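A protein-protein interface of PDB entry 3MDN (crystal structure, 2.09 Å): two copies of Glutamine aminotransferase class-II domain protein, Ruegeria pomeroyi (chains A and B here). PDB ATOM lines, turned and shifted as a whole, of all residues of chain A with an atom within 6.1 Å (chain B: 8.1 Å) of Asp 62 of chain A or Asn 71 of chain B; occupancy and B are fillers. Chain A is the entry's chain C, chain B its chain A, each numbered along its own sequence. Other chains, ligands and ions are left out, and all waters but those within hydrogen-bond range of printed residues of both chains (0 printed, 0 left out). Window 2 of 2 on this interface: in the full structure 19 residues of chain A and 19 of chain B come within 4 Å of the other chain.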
ATOM      1  N   ASP A  44      39.953  22.376 -14.193  1.00  0.00           N
ATOM      2  CA  ASP A  44      39.753  21.850 -12.844  1.00  0.00           C
ATOM      3  C   ASP A  44      38.750  20.687 -12.869  1.00  0.00           C
ATOM      4  O   ASP A  44      39.075  19.615 -13.390  1.00  0.00           O
ATOM      5  CB  ASP A  44      39.319  22.963 -11.870  1.00  0.00           C
ATOM      6  N   GLY A  45      37.545  20.895 -12.327  1.00  0.00           N
ATOM      7  CA  GLY A  45      36.503  19.852 -12.289  1.00  0.00           C
ATOM      8  C   GLY A  45      35.240  20.345 -11.594  1.00  0.00           C
ATOM      9  O   GLY A  45      35.331  21.145 -10.656  1.00  0.00           O
ATOM     10  N   PHE A  46      34.065  19.880 -12.031  1.00  0.00           N
ATOM     11  CA  PHE A  46      32.791  20.419 -11.501  1.00  0.00           C
ATOM     12  C   PHE A  46      31.530  19.533 -11.633  1.00  0.00           C
ATOM     13  O   PHE A  46      31.433  18.704 -12.533  1.00  0.00           O
ATOM     14  CB  PHE A  46      32.480  21.780 -12.136  1.00  0.00           C
ATOM     15  CG  PHE A  46      31.434  22.544 -11.389  1.00  0.00           C
ATOM     16  CD1 PHE A  46      31.760  23.229 -10.220  1.00  0.00           C
ATOM     17  CD2 PHE A  46      30.113  22.527 -11.803  1.00  0.00           C
ATOM     18  CE1 PHE A  46      30.786  23.921  -9.491  1.00  0.00           C
ATOM     19  CE2 PHE A  46      29.129  23.222 -11.084  1.00  0.00           C
ATOM     20  CZ  PHE A  46      29.466  23.924  -9.938  1.00  0.00           C
ATOM     21  N   GLY A  47      30.553  19.756 -10.747  1.00  0.00           N
ATOM     22  CA  GLY A  47      29.255  19.089 -10.843  1.00  0.00           C
ATOM     23  C   GLY A  47      28.184  19.704  -9.974  1.00  0.00           C
ATOM     24  O   GLY A  47      28.483  20.337  -8.971  1.00  0.00           O
ATOM     25  N   LEU A  59      21.640  15.552 -12.475  1.00  0.00           N
ATOM     26  CA  LEU A  59      23.046  15.498 -12.213  1.00  0.00           C
ATOM     27  C   LEU A  59      23.821  16.047 -13.449  1.00  0.00           C
ATOM     28  O   LEU A  59      23.693  15.516 -14.544  1.00  0.00           O
ATOM     29  CB  LEU A  59      23.430  14.054 -11.877  1.00  0.00           C
ATOM     30  CG  LEU A  59      24.929  13.835 -11.609  1.00  0.00           C
ATOM     31  CD1 LEU A  59      25.340  14.678 -10.403  1.00  0.00           C
ATOM     32  CD2 LEU A  59      25.269  12.365 -11.387  1.00  0.00           C
ATOM     33  N   TYR A  60      24.549  17.150 -13.272  1.00  0.00           N
ATOM     34  CA  TYR A  60      25.394  17.706 -14.326  1.00  0.00           C
ATOM     35  C   TYR A  60      26.813  17.688 -13.802  1.00  0.00           C
ATOM     36  O   TYR A  60      27.091  18.286 -12.744  1.00  0.00           O
ATOM     37  CB  TYR A  60      25.016  19.151 -14.636  1.00  0.00           C
ATOM     38  CG  TYR A  60      25.761  19.747 -15.803  1.00  0.00           C
ATOM     39  CD1 TYR A  60      27.107  20.125 -15.696  1.00  0.00           C
ATOM     40  CD2 TYR A  60      25.122  19.927 -17.037  1.00  0.00           C
ATOM     41  CE1 TYR A  60      27.795  20.659 -16.801  1.00  0.00           C
ATOM     42  CE2 TYR A  60      25.784  20.462 -18.124  1.00  0.00           C
ATOM     43  CZ  TYR A  60      27.119  20.822 -18.020  1.00  0.00           C
ATOM     44  OH  TYR A  60      27.754  21.369 -19.125  1.00  0.00           O
ATOM     45  N   ARG A  61      27.726  17.023 -14.507  1.00  0.00           N
ATOM     46  CA  ARG A  61      29.136  17.103 -14.099  1.00  0.00           C
ATOM     47  C   ARG A  61      30.078  16.996 -15.271  1.00  0.00           C
ATOM     48  O   ARG A  61      29.841  16.236 -16.209  1.00  0.00           O
ATOM     49  CB  ARG A  61      29.494  16.075 -12.996  1.00  0.00           C
ATOM     50  CG  ARG A  61      28.815  14.743 -13.128  1.00  0.00           C
ATOM     51  CD  ARG A  61      29.320  13.706 -12.142  1.00  0.00           C
ATOM     52  NE  ARG A  61      28.927  12.386 -12.626  1.00  0.00           N
ATOM     53  CZ  ARG A  61      29.038  11.241 -11.952  1.00  0.00           C
ATOM     54  NH1 ARG A  61      29.548  11.211 -10.720  1.00  0.00           N
ATOM     55  NH2 ARG A  61      28.628  10.116 -12.532  1.00  0.00           N
ATOM     56  N   ASP A  62      31.140  17.799 -15.233  1.00  0.00           N
ATOM     57  CA  ASP A  62      32.142  17.748 -16.287  1.00  0.00           C
ATOM     58  C   ASP A  62      33.518  18.155 -15.816  1.00  0.00           C
ATOM     59  O   ASP A  62      33.666  18.815 -14.782  1.00  0.00           O
ATOM     60  CB  ASP A  62      31.720  18.574 -17.493  1.00  0.00           C
ATOM     61  CG  ASP A  62      32.034  17.875 -18.798  1.00  0.00           C
ATOM     62  OD1 ASP A  62      33.064  17.168 -18.848  1.00  0.00           O
ATOM     63  OD2 ASP A  62      31.246  18.020 -19.757  1.00  0.00           O
ATOM     64  N   VAL A  63      34.518  17.754 -16.604  1.00  0.00           N
ATOM     65  CA  VAL A  63      35.912  17.803 -16.193  1.00  0.00           C
ATOM     66  C   VAL A  63      36.603  19.089 -16.613  1.00  0.00           C
ATOM     67  O   VAL A  63      37.813  19.103 -16.838  1.00  0.00           O
ATOM     68  CB  VAL A  63      36.722  16.571 -16.722  1.00  0.00           C
ATOM     69  CG1 VAL A  63      36.140  15.258 -16.190  1.00  0.00           C
ATOM     70  CG2 VAL A  63      36.770  16.554 -18.242  1.00  0.00           C
ATOM     71  N   TYR A  64      35.854  20.174 -16.744  1.00  0.00           N
ATOM     72  CA  TYR A  64      36.522  21.448 -16.999  1.00  0.00           C
ATOM     73  C   TYR A  64      35.923  22.677 -16.306  1.00  0.00           C
ATOM     74  O   TYR A  64      34.752  22.663 -15.904  1.00  0.00           O
ATOM     75  CB  TYR A  64      36.850  21.655 -18.496  1.00  0.00           C
ATOM     76  CG  TYR A  64      35.769  22.182 -19.421  1.00  0.00           C
ATOM     77  CD1 TYR A  64      35.898  23.449 -20.003  1.00  0.00           C
ATOM     78  CD2 TYR A  64      34.670  21.398 -19.789  1.00  0.00           C
ATOM     79  CE1 TYR A  64      34.939  23.945 -20.887  1.00  0.00           C
ATOM     80  CE2 TYR A  64      33.702  21.888 -20.681  1.00  0.00           C
ATOM     81  CZ  TYR A  64      33.848  23.163 -21.225  1.00  0.00           C
ATOM     82  OH  TYR A  64      32.918  23.674 -22.101  1.00  0.00           O
ATOM     83  N   PRO A  65      36.753  23.730 -16.144  1.00  0.00           N
ATOM     84  CA  PRO A  65      36.481  24.815 -15.197  1.00  0.00           C
ATOM     85  C   PRO A  65      35.099  25.440 -15.355  1.00  0.00           C
ATOM     86  O   PRO A  65      34.760  25.960 -16.430  1.00  0.00           O
ATOM     87  CB  PRO A  65      37.594  25.848 -15.490  1.00  0.00           C
ATOM     88  CG  PRO A  65      38.155  25.468 -16.838  1.00  0.00           C
ATOM     89  CD  PRO A  65      38.001  23.971 -16.901  1.00  0.00           C
ATOM     90  N   ASP A  69      32.441  26.431 -19.227  1.00  0.00           N
ATOM     91  CA  ASP A  69      31.446  25.564 -19.841  1.00  0.00           C
ATOM     92  C   ASP A  69      30.181  26.370 -20.073  1.00  0.00           C
ATOM     93  O   ASP A  69      29.403  26.547 -19.146  1.00  0.00           O
ATOM     94  CB  ASP A  69      31.157  24.443 -18.822  1.00  0.00           C
ATOM     95  CG  ASP A  69      30.426  23.254 -19.415  1.00  0.00           C
ATOM     96  OD1 ASP A  69      29.760  23.406 -20.467  1.00  0.00           O
ATOM     97  OD2 ASP A  69      30.528  22.159 -18.812  1.00  0.00           O
ATOM     98  N   ASN A  99      32.798   7.941 -13.757  1.00  0.00           N
ATOM     99  CA  ASN A  99      33.498   9.225 -13.661  1.00  0.00           C
ATOM    100  C   ASN A  99      33.874   9.625 -12.213  1.00  0.00           C
ATOM    101  O   ASN A  99      33.381   9.056 -11.239  1.00  0.00           O
ATOM    102  CB  ASN A  99      32.691  10.323 -14.371  1.00  0.00           C
ATOM    103  CG  ASN A  99      33.184  11.731 -14.050  1.00  0.00           C
ATOM    104  OD1 ASN A  99      32.457  12.518 -13.440  1.00  0.00           O
ATOM    105  ND2 ASN A  99      34.419  12.057 -14.469  1.00  0.00           N
ATOM    106  N   CYS A 101      34.052  13.027 -10.933  1.00  0.00           N
ATOM    107  CA  CYS A 101      33.520  14.304 -10.432  1.00  0.00           C
ATOM    108  C   CYS A 101      32.334  14.014  -9.535  1.00  0.00           C
ATOM    109  O   CYS A 101      31.625  13.044  -9.768  1.00  0.00           O
ATOM    110  CB  CYS A 101      33.155  15.268 -11.570  1.00  0.00           C
ATOM    111  SG  CYS A 101      34.652  15.925 -12.426  1.00  0.00           S
ATOM    112  N   TYR B  60      21.674  25.031 -24.680  1.00  0.00           N
ATOM    113  CA  TYR B  60      22.625  23.968 -24.421  1.00  0.00           C
ATOM    114  C   TYR B  60      23.014  23.405 -25.759  1.00  0.00           C
ATOM    115  O   TYR B  60      22.136  22.938 -26.519  1.00  0.00           O
ATOM    116  CB  TYR B  60      22.013  22.848 -23.560  1.00  0.00           C
ATOM    117  CG  TYR B  60      22.981  21.712 -23.213  1.00  0.00           C
ATOM    118  CD1 TYR B  60      23.512  20.882 -24.206  1.00  0.00           C
ATOM    119  CD2 TYR B  60      23.372  21.482 -21.898  1.00  0.00           C
ATOM    120  CE1 TYR B  60      24.402  19.853 -23.902  1.00  0.00           C
ATOM    121  CE2 TYR B  60      24.266  20.449 -21.570  1.00  0.00           C
ATOM    122  CZ  TYR B  60      24.783  19.642 -22.579  1.00  0.00           C
ATOM    123  OH  TYR B  60      25.666  18.617 -22.252  1.00  0.00           O
ATOM    124  N   ASP B  62      26.501  21.198 -27.828  1.00  0.00           N
ATOM    125  CA  ASP B  62      27.723  20.449 -27.678  1.00  0.00           C
ATOM    126  C   ASP B  62      27.955  19.648 -28.945  1.00  0.00           C
ATOM    127  O   ASP B  62      27.017  19.409 -29.725  1.00  0.00           O
ATOM    128  CB  ASP B  62      27.567  19.492 -26.502  1.00  0.00           C
ATOM    129  CG  ASP B  62      28.852  19.320 -25.712  1.00  0.00           C
ATOM    130  OD1 ASP B  62      29.918  19.773 -26.197  1.00  0.00           O
ATOM    131  OD2 ASP B  62      28.789  18.731 -24.603  1.00  0.00           O
ATOM    132  N   TYR B  64      28.963  16.520 -28.901  1.00  0.00           N
ATOM    133  CA  TYR B  64      28.891  15.099 -28.554  1.00  0.00           C
ATOM    134  C   TYR B  64      27.546  14.513 -28.994  1.00  0.00           C
ATOM    135  O   TYR B  64      26.546  15.235 -29.044  1.00  0.00           O
ATOM    136  CB  TYR B  64      29.145  14.891 -27.048  1.00  0.00           C
ATOM    137  CG  TYR B  64      30.577  15.179 -26.630  1.00  0.00           C
ATOM    138  CD1 TYR B  64      31.566  14.201 -26.740  1.00  0.00           C
ATOM    139  CD2 TYR B  64      30.947  16.434 -26.134  1.00  0.00           C
ATOM    140  CE1 TYR B  64      32.883  14.459 -26.366  1.00  0.00           C
ATOM    141  CE2 TYR B  64      32.274  16.701 -25.758  1.00  0.00           C
ATOM    142  CZ  TYR B  64      33.228  15.705 -25.878  1.00  0.00           C
ATOM    143  OH  TYR B  64      34.533  15.944 -25.508  1.00  0.00           O
ATOM    144  N   ALA B  66      24.000  13.269 -28.982  1.00  0.00           N
ATOM    145  CA  ALA B  66      22.905  13.294 -28.008  1.00  0.00           C
ATOM    146  C   ALA B  66      22.795  11.968 -27.243  1.00  0.00           C
ATOM    147  O   ALA B  66      22.650  11.953 -26.014  1.00  0.00           O
ATOM    148  CB  ALA B  66      21.592  13.613 -28.699  1.00  0.00           C
ATOM    149  N   SER B  68      24.996   9.975 -26.434  1.00  0.00           N
ATOM    150  CA  SER B  68      26.146   9.714 -25.573  1.00  0.00           C
ATOM    151  C   SER B  68      26.717  10.907 -24.792  1.00  0.00           C
ATOM    152  O   SER B  68      27.930  10.982 -24.552  1.00  0.00           O
ATOM    153  CB  SER B  68      27.253   9.068 -26.398  1.00  0.00           C
ATOM    154  OG  SER B  68      27.383   7.691 -26.075  1.00  0.00           O
ATOM    155  N   ASP B  69      25.850  11.824 -24.379  1.00  0.00           N
ATOM    156  CA  ASP B  69      26.231  12.914 -23.481  1.00  0.00           C
ATOM    157  C   ASP B  69      25.314  12.840 -22.252  1.00  0.00           C
ATOM    158  O   ASP B  69      24.137  13.167 -22.348  1.00  0.00           O
ATOM    159  CB  ASP B  69      26.082  14.272 -24.195  1.00  0.00           C
ATOM    160  CG  ASP B  69      26.205  15.459 -23.249  1.00  0.00           C
ATOM    161  OD1 ASP B  69      26.251  15.238 -22.017  1.00  0.00           O
ATOM    162  OD2 ASP B  69      26.265  16.614 -23.738  1.00  0.00           O
ATOM    163  N   PRO B  70      25.846  12.417 -21.095  1.00  0.00           N
ATOM    164  CA  PRO B  70      24.947  12.179 -19.956  1.00  0.00           C
ATOM    165  C   PRO B  70      24.381  13.471 -19.341  1.00  0.00           C
ATOM    166  O   PRO B  70      23.341  13.444 -18.696  1.00  0.00           O
ATOM    167  CB  PRO B  70      25.832  11.410 -18.954  1.00  0.00           C
ATOM    168  CG  PRO B  70      27.247  11.812 -19.299  1.00  0.00           C
ATOM    169  CD  PRO B  70      27.276  12.281 -20.739  1.00  0.00           C
ATOM    170  N   ASN B  71      25.060  14.594 -19.548  1.00  0.00           N
ATOM    171  CA  ASN B  71      24.587  15.876 -19.052  1.00  0.00           C
ATOM    172  C   ASN B  71      23.345  16.331 -19.845  1.00  0.00           C
ATOM    173  O   ASN B  71      22.323  16.762 -19.276  1.00  0.00           O
ATOM    174  CB  ASN B  71      25.709  16.921 -19.146  1.00  0.00           C
ATOM    175  CG  ASN B  71      26.858  16.652 -18.163  1.00  0.00           C
ATOM    176  OD1 ASN B  71      26.641  16.145 -17.071  1.00  0.00           O
ATOM    177  ND2 ASN B  71      28.082  17.007 -18.557  1.00  0.00           N
ATOM    178  N   LEU B  72      23.423  16.220 -21.170  1.00  0.00           N
ATOM    179  CA  LEU B  72      22.267  16.536 -21.958  1.00  0.00           C
ATOM    180  C   LEU B  72      21.099  15.649 -21.525  1.00  0.00           C
ATOM    181  O   LEU B  72      19.951  16.097 -21.411  1.00  0.00           O
ATOM    182  CB  LEU B  72      22.542  16.334 -23.444  1.00  0.00           C
ATOM    183  CG  LEU B  72      21.181  16.271 -24.138  1.00  0.00           C
ATOM    184  CD1 LEU B  72      20.653  17.686 -24.333  1.00  0.00           C
ATOM    185  CD2 LEU B  72      21.308  15.522 -25.439  1.00  0.00           C
ATOM    186  N   ARG B  73      21.394  14.386 -21.286  1.00  0.00           N
ATOM    187  CA  ARG B  73      20.374  13.460 -20.867  1.00  0.00           C
ATOM    188  C   ARG B  73      19.701  13.917 -19.563  1.00  0.00           C
ATOM    189  O   ARG B  73      18.467  13.895 -19.422  1.00  0.00           O
ATOM    190  CB  ARG B  73      20.976  12.064 -20.727  1.00  0.00           C
ATOM    191  CG  ARG B  73      19.944  10.997 -20.404  1.00  0.00           C
ATOM    192  CD  ARG B  73      20.462   9.562 -20.689  1.00  0.00           C
ATOM    193  NE  ARG B  73      19.349   8.657 -21.026  1.00  0.00           N
ATOM    194  CZ  ARG B  73      18.428   8.922 -21.959  1.00  0.00           C
ATOM    195  NH1 ARG B  73      18.479  10.055 -22.643  1.00  0.00           N
ATOM    196  NH2 ARG B  73      17.449   8.066 -22.211  1.00  0.00           N
ATOM    197  N   ALA B  74      20.515  14.335 -18.602  1.00  0.00           N
ATOM    198  CA  ALA B  74      19.958  14.827 -17.354  1.00  0.00           C
ATOM    199  C   ALA B  74      19.147  16.119 -17.547  1.00  0.00           C
ATOM    200  O   ALA B  74      18.102  16.264 -16.941  1.00  0.00           O
ATOM    201  CB  ALA B  74      21.062  15.006 -16.309  1.00  0.00           C
ATOM    202  N   VAL B  75      19.634  17.057 -18.357  1.00  0.00           N
ATOM    203  CA  VAL B  75      18.858  18.252 -18.660  1.00  0.00           C
ATOM    204  C   VAL B  75      17.485  17.905 -19.312  1.00  0.00           C
ATOM    205  O   VAL B  75      16.433  18.401 -18.877  1.00  0.00           O
ATOM    206  CB  VAL B  75      19.641  19.235 -19.558  1.00  0.00           C
ATOM    207  CG1 VAL B  75      18.704  20.302 -20.146  1.00  0.00           C
ATOM    208  CG2 VAL B  75      20.798  19.873 -18.796  1.00  0.00           C
ATOM    209  N   ALA B  76      17.492  17.022 -20.317  1.00  0.00           N
ATOM    210  CA  ALA B  76      16.248  16.701 -21.047  1.00  0.00           C
ATOM    211  C   ALA B  76      15.299  15.890 -20.193  1.00  0.00           C
ATOM    212  O   ALA B  76      14.092  15.923 -20.405  1.00  0.00           O
ATOM    213  CB  ALA B  76      16.532  15.974 -22.369  1.00  0.00           C
ATOM    214  N   HIS B  77      15.832  15.175 -19.217  1.00  0.00           N
ATOM    215  CA  HIS B  77      15.000  14.346 -18.359  1.00  0.00           C
ATOM    216  C   HIS B  77      14.417  15.179 -17.201  1.00  0.00           C
ATOM    217  O   HIS B  77      13.390  14.805 -16.631  1.00  0.00           O
ATOM    218  CB  HIS B  77      15.816  13.141 -17.859  1.00  0.00           C
ATOM    219  CG  HIS B  77      15.103  12.232 -16.892  1.00  0.00           C
ATOM    220  ND1 HIS B  77      13.977  11.509 -17.228  1.00  0.00           N
ATOM    221  CD2 HIS B  77      15.428  11.846 -15.629  1.00  0.00           C
ATOM    222  CE1 HIS B  77      13.603  10.767 -16.198  1.00  0.00           C
ATOM    223  NE2 HIS B  77      14.465  10.955 -15.216  1.00  0.00           N
ATOM    224  N   HIS B  78      15.047  16.311 -16.868  1.00  0.00           N
ATOM    225  CA  HIS B  78      14.640  17.050 -15.675  1.00  0.00           C
ATOM    226  C   HIS B  78      14.047  18.445 -15.921  1.00  0.00           C
ATOM    227  O   HIS B  78      13.354  18.980 -15.066  1.00  0.00           O
ATOM    228  CB  HIS B  78      15.810  17.162 -14.660  1.00  0.00           C
ATOM    229  CG  HIS B  78      16.018  15.926 -13.825  1.00  0.00           C
ATOM    230  ND1 HIS B  78      16.898  14.920 -14.178  1.00  0.00           N
ATOM    231  CD2 HIS B  78      15.451  15.535 -12.661  1.00  0.00           C
ATOM    232  CE1 HIS B  78      16.860  13.966 -13.266  1.00  0.00           C
ATOM    233  NE2 HIS B  78      15.995  14.319 -12.333  1.00  0.00           N
ATOM    234  N   VAL B  79      14.348  19.056 -17.054  1.00  0.00           N
ATOM    235  CA  VAL B  79      13.869  20.403 -17.285  1.00  0.00           C
ATOM    236  C   VAL B  79      12.547  20.337 -18.058  1.00  0.00           C
ATOM    237  O   VAL B  79      12.435  19.599 -19.034  1.00  0.00           O
ATOM    238  CB  VAL B  79      14.917  21.251 -18.065  1.00  0.00           C
ATOM    239  CG1 VAL B  79      14.328  22.624 -18.530  1.00  0.00           C
ATOM    240  CG2 VAL B  79      16.156  21.418 -17.215  1.00  0.00           C
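Asp 62 of chain A touches just one residue of chain B: Asn 71. Printed residues of chain B within 4 Å of Arg 61 of chain A: Asn 71 (2.9 Å). Of the printed residues of chain A, Tyr 60 of chain B touches Tyr 60. Of the printed residues of chain B, Leu 59 of chain A touches Asn 71 (3.9 Å) and Ala 74 (3.2 Å). Ala 66 of chain B touches none of the printed residues of chain A. Ser 68 of chain B touches none of the printed residues of chain A.
The side-chain hydroxyl of Tyr 60 of chain B lies within hydrogen-bond range of the side-chain carboxylate of Asp 69 of chain B (2.6 Å). The side-chain hydroxyl of Tyr 60 of chain B lies within hydrogen-bond range of the backbone NH of Leu 72 of chain B (3.5 Å). The backbone NH (N) of Asn 71 of chain B is in hydrogen-bond range of the side-chain carboxylate (OD1) of Asp 69 of chain B (2.8 Å). ND1 of His 78 of chain B is in hydrogen-bond range of O of Ala 74 of chain B, 3.3 Å away. The backbone carbonyl oxygen (O) of Phe 46 of chain A lies within hydrogen-bond range of the backbone NH (N) of Asp 62 of chain A (2.9 Å). The side-chain carboxylate of Asp 69 of chain A is in hydrogen-bond range of the side-chain hydroxyl of Tyr 60 of chain A (2.9 Å).
Of the 14 printed residues of chain A, 4 touch a printed residue of chain B. Hydrophobic or aromatic side chains of chain A within 4 Å of the printed part of chain B: Tyr 60. Of the 16 printed residues of chain B, 3 touch a printed residue of chain A. Hydrophobic or aromatic side chains of chain B that line the printed part of chain A: Tyr 60 and Ala 74. Along chain B the printed residues that touch a printed residue of chain A span positions 60 to 74. Among the printed residues, no Asp or Glu carboxylate lies within 4 Å of a Lys or Arg side-chain nitrogen of the other chain.
Among the printed residues, merely in contact across the chains: Leu 59 of chain A with Ala 74 of chain B (3.2 Å), Tyr 60 of chain A with Asn 71 of chain B (3.4 Å), Asp 62 of chain A with Asn 71 of chain B (3.5 Å), Tyr 60 of chain A with Tyr 60 of chain B (3.8 Å) and Leu 59 of chain A with Asn 71 of chain B (3.9 Å).
Tyr 60 of chain B touches its own counterpart, Tyr 60 of chain A. 4 positions are printed for both chains.
The backbone NH of Arg 61 of chain A sits at hydrogen-bond distance from the side-chain amide oxygen of Asn 71 of chain B (2.9 Å).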
